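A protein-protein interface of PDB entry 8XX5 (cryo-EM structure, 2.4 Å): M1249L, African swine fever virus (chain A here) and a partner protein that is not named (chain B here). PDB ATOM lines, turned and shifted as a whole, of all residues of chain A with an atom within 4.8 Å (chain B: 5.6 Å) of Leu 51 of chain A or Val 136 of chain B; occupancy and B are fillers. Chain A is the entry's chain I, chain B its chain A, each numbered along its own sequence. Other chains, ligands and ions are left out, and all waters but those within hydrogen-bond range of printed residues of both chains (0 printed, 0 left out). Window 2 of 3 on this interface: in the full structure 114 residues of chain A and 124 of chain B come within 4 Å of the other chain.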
ATOM      1  N   LYS A  41     -22.318 -12.578  13.926  1.00  0.00           N
ATOM      2  CA  LYS A  41     -23.044 -12.006  12.802  1.00  0.00           C
ATOM      3  C   LYS A  41     -22.157 -11.957  11.570  1.00  0.00           C
ATOM      4  O   LYS A  41     -20.980 -11.597  11.653  1.00  0.00           O
ATOM      5  CB  LYS A  41     -23.550 -10.596  13.133  1.00  0.00           C
ATOM      6  CG  LYS A  41     -24.591 -10.074  12.162  1.00  0.00           C
ATOM      7  CD  LYS A  41     -25.770 -11.024  12.085  1.00  0.00           C
ATOM      8  CE  LYS A  41     -26.668 -10.701  10.909  1.00  0.00           C
ATOM      9  NZ  LYS A  41     -26.854  -9.237  10.744  1.00  0.00           N
ATOM     10  N   GLU A  42     -22.729 -12.321  10.426  1.00  0.00           N
ATOM     11  CA  GLU A  42     -22.060 -12.157   9.146  1.00  0.00           C
ATOM     12  C   GLU A  42     -22.365 -10.775   8.586  1.00  0.00           C
ATOM     13  O   GLU A  42     -23.513 -10.324   8.601  1.00  0.00           O
ATOM     14  CB  GLU A  42     -22.493 -13.236   8.153  1.00  0.00           C
ATOM     15  CG  GLU A  42     -22.092 -14.643   8.554  1.00  0.00           C
ATOM     16  CD  GLU A  42     -22.207 -15.632   7.410  1.00  0.00           C
ATOM     17  OE1 GLU A  42     -21.677 -16.755   7.538  1.00  0.00           O
ATOM     18  OE2 GLU A  42     -22.827 -15.287   6.383  1.00  0.00           O
ATOM     19  N   ILE A  43     -21.325 -10.105   8.096  1.00  0.00           N
ATOM     20  CA  ILE A  43     -21.415  -8.728   7.639  1.00  0.00           C
ATOM     21  C   ILE A  43     -20.868  -8.639   6.221  1.00  0.00           C
ATOM     22  O   ILE A  43     -20.267  -9.577   5.698  1.00  0.00           O
ATOM     23  CB  ILE A  43     -20.653  -7.754   8.561  1.00  0.00           C
ATOM     24  CG1 ILE A  43     -19.145  -7.917   8.356  1.00  0.00           C
ATOM     25  CG2 ILE A  43     -21.023  -7.985  10.015  1.00  0.00           C
ATOM     26  CD1 ILE A  43     -18.301  -7.097   9.298  1.00  0.00           C
ATOM     27  N   LEU A  45     -18.544  -5.685   3.992  1.00  0.00           N
ATOM     28  CA  LEU A  45     -17.855  -4.409   4.043  1.00  0.00           C
ATOM     29  C   LEU A  45     -18.423  -3.470   2.982  1.00  0.00           C
ATOM     30  O   LEU A  45     -19.198  -3.870   2.109  1.00  0.00           O
ATOM     31  CB  LEU A  45     -16.351  -4.598   3.859  1.00  0.00           C
ATOM     32  CG  LEU A  45     -15.603  -5.177   5.065  1.00  0.00           C
ATOM     33  CD1 LEU A  45     -14.113  -4.883   4.973  1.00  0.00           C
ATOM     34  CD2 LEU A  45     -16.177  -4.656   6.376  1.00  0.00           C
ATOM     35  N   THR A  49     -16.785  -7.327   0.309  1.00  0.00           N
ATOM     36  CA  THR A  49     -16.287  -8.574   0.875  1.00  0.00           C
ATOM     37  C   THR A  49     -17.168  -9.027   2.032  1.00  0.00           C
ATOM     38  O   THR A  49     -17.643  -8.216   2.831  1.00  0.00           O
ATOM     39  CB  THR A  49     -14.841  -8.421   1.349  1.00  0.00           C
ATOM     40  OG1 THR A  49     -14.531  -9.462   2.282  1.00  0.00           O
ATOM     41  CG2 THR A  49     -14.634  -7.083   2.022  1.00  0.00           C
ATOM     42  N   HIS A  50     -17.382 -10.336   2.117  1.00  0.00           N
ATOM     43  CA  HIS A  50     -18.270 -10.933   3.104  1.00  0.00           C
ATOM     44  C   HIS A  50     -17.436 -11.501   4.246  1.00  0.00           C
ATOM     45  O   HIS A  50     -16.554 -12.337   4.019  1.00  0.00           O
ATOM     46  CB  HIS A  50     -19.122 -12.026   2.460  1.00  0.00           C
ATOM     47  CG  HIS A  50     -20.147 -12.617   3.375  1.00  0.00           C
ATOM     48  ND1 HIS A  50     -20.994 -11.846   4.141  1.00  0.00           N
ATOM     49  CD2 HIS A  50     -20.469 -13.904   3.639  1.00  0.00           C
ATOM     50  CE1 HIS A  50     -21.791 -12.634   4.841  1.00  0.00           C
ATOM     51  NE2 HIS A  50     -21.493 -13.888   4.556  1.00  0.00           N
ATOM     52  N   LEU A  51     -17.713 -11.048   5.466  1.00  0.00           N
ATOM     53  CA  LEU A  51     -17.009 -11.510   6.652  1.00  0.00           C
ATOM     54  C   LEU A  51     -18.006 -11.773   7.771  1.00  0.00           C
ATOM     55  O   LEU A  51     -19.203 -11.503   7.649  1.00  0.00           O
ATOM     56  CB  LEU A  51     -15.956 -10.496   7.119  1.00  0.00           C
ATOM     57  CG  LEU A  51     -14.836 -10.126   6.146  1.00  0.00           C
ATOM     58  CD1 LEU A  51     -15.130  -8.798   5.475  1.00  0.00           C
ATOM     59  CD2 LEU A  51     -13.503 -10.082   6.869  1.00  0.00           C
ATOM     60  N   ALA A  52     -17.492 -12.311   8.871  1.00  0.00           N
ATOM     61  CA  ALA A  52     -18.274 -12.557  10.072  1.00  0.00           C
ATOM     62  C   ALA A  52     -17.523 -12.006  11.272  1.00  0.00           C
ATOM     63  O   ALA A  52     -16.299 -12.130  11.358  1.00  0.00           O
ATOM     64  CB  ALA A  52     -18.554 -14.050  10.267  1.00  0.00           C
ATOM     65  N   VAL A  53     -18.257 -11.391  12.193  1.00  0.00           N
ATOM     66  CA  VAL A  53     -17.658 -10.817  13.394  1.00  0.00           C
ATOM     67  C   VAL A  53     -18.137 -11.604  14.609  1.00  0.00           C
ATOM     68  O   VAL A  53     -19.246 -12.155  14.590  1.00  0.00           O
ATOM     69  CB  VAL A  53     -17.999  -9.325  13.527  1.00  0.00           C
ATOM     70  CG1 VAL A  53     -17.276  -8.523  12.458  1.00  0.00           C
ATOM     71  CG2 VAL A  53     -19.500  -9.112  13.436  1.00  0.00           C
ATOM     72  N   CYS B 102      -9.367 -11.853  10.858  1.00  0.00           N
ATOM     73  CA  CYS B 102     -10.696 -11.520  10.372  1.00  0.00           C
ATOM     74  C   CYS B 102     -11.521 -12.742   9.995  1.00  0.00           C
ATOM     75  O   CYS B 102     -12.693 -12.589   9.633  1.00  0.00           O
ATOM     76  CB  CYS B 102     -10.603 -10.580   9.164  1.00  0.00           C
ATOM     77  SG  CYS B 102      -9.702 -11.264   7.762  1.00  0.00           S
ATOM     78  N   ALA B 104     -11.224 -14.654   7.400  1.00  0.00           N
ATOM     79  CA  ALA B 104     -11.264 -14.946   5.980  1.00  0.00           C
ATOM     80  C   ALA B 104     -10.340 -16.120   5.657  1.00  0.00           C
ATOM     81  O   ALA B 104      -9.349 -16.350   6.353  1.00  0.00           O
ATOM     82  CB  ALA B 104     -10.855 -13.719   5.171  1.00  0.00           C
ATOM     83  N   CYS B 134      -2.973 -12.092   4.387  1.00  0.00           N
ATOM     84  CA  CYS B 134      -4.402 -11.962   4.154  1.00  0.00           C
ATOM     85  C   CYS B 134      -4.676 -10.819   3.188  1.00  0.00           C
ATOM     86  O   CYS B 134      -4.044  -9.763   3.255  1.00  0.00           O
ATOM     87  CB  CYS B 134      -5.131 -11.721   5.475  1.00  0.00           C
ATOM     88  SG  CYS B 134      -6.924 -11.864   5.375  1.00  0.00           S
ATOM     89  N   TYR B 135      -5.620 -11.032   2.277  1.00  0.00           N
ATOM     90  CA  TYR B 135      -5.990 -10.001   1.319  1.00  0.00           C
ATOM     91  C   TYR B 135      -7.104  -9.098   1.830  1.00  0.00           C
ATOM     92  O   TYR B 135      -7.540  -8.202   1.100  1.00  0.00           O
ATOM     93  CB  TYR B 135      -6.390 -10.638  -0.018  1.00  0.00           C
ATOM     94  CG  TYR B 135      -7.862 -10.947  -0.171  1.00  0.00           C
ATOM     95  CD1 TYR B 135      -8.474 -11.927   0.598  1.00  0.00           C
ATOM     96  CD2 TYR B 135      -8.640 -10.261  -1.095  1.00  0.00           C
ATOM     97  CE1 TYR B 135      -9.821 -12.213   0.453  1.00  0.00           C
ATOM     98  CE2 TYR B 135      -9.984 -10.536  -1.246  1.00  0.00           C
ATOM     99  CZ  TYR B 135     -10.571 -11.512  -0.470  1.00  0.00           C
ATOM    100  OH  TYR B 135     -11.910 -11.787  -0.621  1.00  0.00           O
ATOM    101  N   VAL B 136      -7.563  -9.303   3.064  1.00  0.00           N
ATOM    102  CA  VAL B 136      -8.606  -8.474   3.656  1.00  0.00           C
ATOM    103  C   VAL B 136      -7.987  -7.527   4.675  1.00  0.00           C
ATOM    104  O   VAL B 136      -8.161  -6.307   4.591  1.00  0.00           O
ATOM    105  CB  VAL B 136      -9.700  -9.338   4.310  1.00  0.00           C
ATOM    106  CG1 VAL B 136     -10.725  -8.456   5.008  1.00  0.00           C
ATOM    107  CG2 VAL B 136     -10.370 -10.219   3.275  1.00  0.00           C
ATOM    108  N   CYS B 137      -7.262  -8.083   5.643  1.00  0.00           N
ATOM    109  CA  CYS B 137      -6.686  -7.308   6.732  1.00  0.00           C
ATOM    110  C   CYS B 137      -5.168  -7.218   6.673  1.00  0.00           C
ATOM    111  O   CYS B 137      -4.564  -6.617   7.568  1.00  0.00           O
ATOM    112  CB  CYS B 137      -7.118  -7.899   8.079  1.00  0.00           C
ATOM    113  SG  CYS B 137      -6.400  -9.512   8.434  1.00  0.00           S
ATOM    114  N   LYS B 138      -4.537  -7.805   5.653  1.00  0.00           N
ATOM    115  CA  LYS B 138      -3.093  -7.699   5.434  1.00  0.00           C
ATOM    116  C   LYS B 138      -2.286  -8.260   6.601  1.00  0.00           C
ATOM    117  O   LYS B 138      -1.188  -7.781   6.895  1.00  0.00           O
ATOM    118  CB  LYS B 138      -2.677  -6.252   5.146  1.00  0.00           C
ATOM    119  CG  LYS B 138      -2.857  -5.822   3.695  1.00  0.00           C
ATOM    120  CD  LYS B 138      -4.306  -5.486   3.384  1.00  0.00           C
ATOM    121  CE  LYS B 138      -4.852  -4.450   4.353  1.00  0.00           C
ATOM    122  NZ  LYS B 138      -6.136  -3.864   3.876  1.00  0.00           N
ATOM    123  N   ARG B 176     -15.427 -16.098  13.354  1.00  0.00           N
ATOM    124  CA  ARG B 176     -15.322 -15.168  12.240  1.00  0.00           C
ATOM    125  C   ARG B 176     -15.390 -15.859  10.886  1.00  0.00           C
ATOM    126  O   ARG B 176     -15.335 -15.180   9.856  1.00  0.00           O
ATOM    127  CB  ARG B 176     -14.026 -14.361  12.353  1.00  0.00           C
ATOM    128  CG  ARG B 176     -14.072 -13.291  13.429  1.00  0.00           C
ATOM    129  CD  ARG B 176     -12.818 -12.442  13.428  1.00  0.00           C
ATOM    130  NE  ARG B 176     -11.676 -13.161  13.981  1.00  0.00           N
ATOM    131  CZ  ARG B 176     -11.160 -12.936  15.181  1.00  0.00           C
ATOM    132  NH1 ARG B 176     -11.668 -12.024  15.992  1.00  0.00           N
ATOM    133  NH2 ARG B 176     -10.106 -13.645  15.576  1.00  0.00           N
ATOM    134  N   THR B 178     -17.196 -17.451   7.847  1.00  0.00           N
ATOM    135  CA  THR B 178     -18.513 -17.414   7.236  1.00  0.00           C
ATOM    136  C   THR B 178     -18.945 -18.813   6.809  1.00  0.00           C
ATOM    137  O   THR B 178     -18.126 -19.716   6.618  1.00  0.00           O
ATOM    138  CB  THR B 178     -18.525 -16.479   6.025  1.00  0.00           C
ATOM    139  OG1 THR B 178     -17.386 -16.746   5.199  1.00  0.00           O
ATOM    140  CG2 THR B 178     -18.489 -15.028   6.473  1.00  0.00           C
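NE2 of His 50 of chain A is in hydrogen-bond range of OE2 of Glu 42 of chain A (2.7 Å). The backbone carbonyl oxygen (O) of Ile 43 of chain A sits at hydrogen-bond distance from a ring nitrogen (ND1) of His 50 of chain A (2.8 Å). The backbone carbonyl oxygen of Leu 51 of chain A lies within hydrogen-bond range of the backbone NH of Ile 43 of chain A. SG of Cys 102 of chain B sits close to N of Ala 104 of chain B (3.7 Å). SG of Cys 134 of chain B lies close to N of Val 136 of chain B (3.5 Å). The backbone carbonyl oxygen (O) of Val 136 of chain B sits at hydrogen-bond distance from the side-chain amino group (NZ) of Lys 138 of chain B.
Among the printed residues, pairs that only touch across the chains: Glu 42 of chain A with Thr 178 of chain B (3.2 Å), Ala 52 of chain A with Arg 176 of chain B (3.3 Å), Leu 51 of chain A with Thr 178 of chain B (3.5 Å), His 50 of chain A with Thr 178 of chain B (3.6 Å), Leu 51 of chain A with Val 136 of chain B (3.7 Å), Leu 51 of chain A with Cys 102 of chain B (3.7 Å) and Ala 52 of chain A with Thr 178 of chain B (3.8 Å).
Of the printed residues of chain B, His 50 of chain A touches Thr 178 (3.6 Å). Printed residues of chain A within 4 Å of Cys 102 of chain B: Leu 51. Tyr 135 of chain B touches none of the printed residues of chain A. Val 136 of chain B touches just one residue of chain A: Leu 51. Printed residues of chain A within 4 Å of Thr 178 of chain B: Glu 42 (3.2 Å), His 50 (3.6 Å), Leu 51 (3.5 Å) and Ala 52 (3.8 Å). The nearest printed residue of chain B that does not touch His 50 of chain A is Ala 104 of chain B (6.0 Å).
Hydrophobic or aromatic side chains of chain A within 4 Å of the printed part of chain B: His 50, Leu 51 and Ala 52. Along chain A the printed residues that touch a printed residue of chain B span positions 42 to 52. Of the 9 printed residues of chain B, 4 touch a printed residue of chain A. Hydrophobic or aromatic side chains of chain B that line the printed part of chain A: Val 136.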
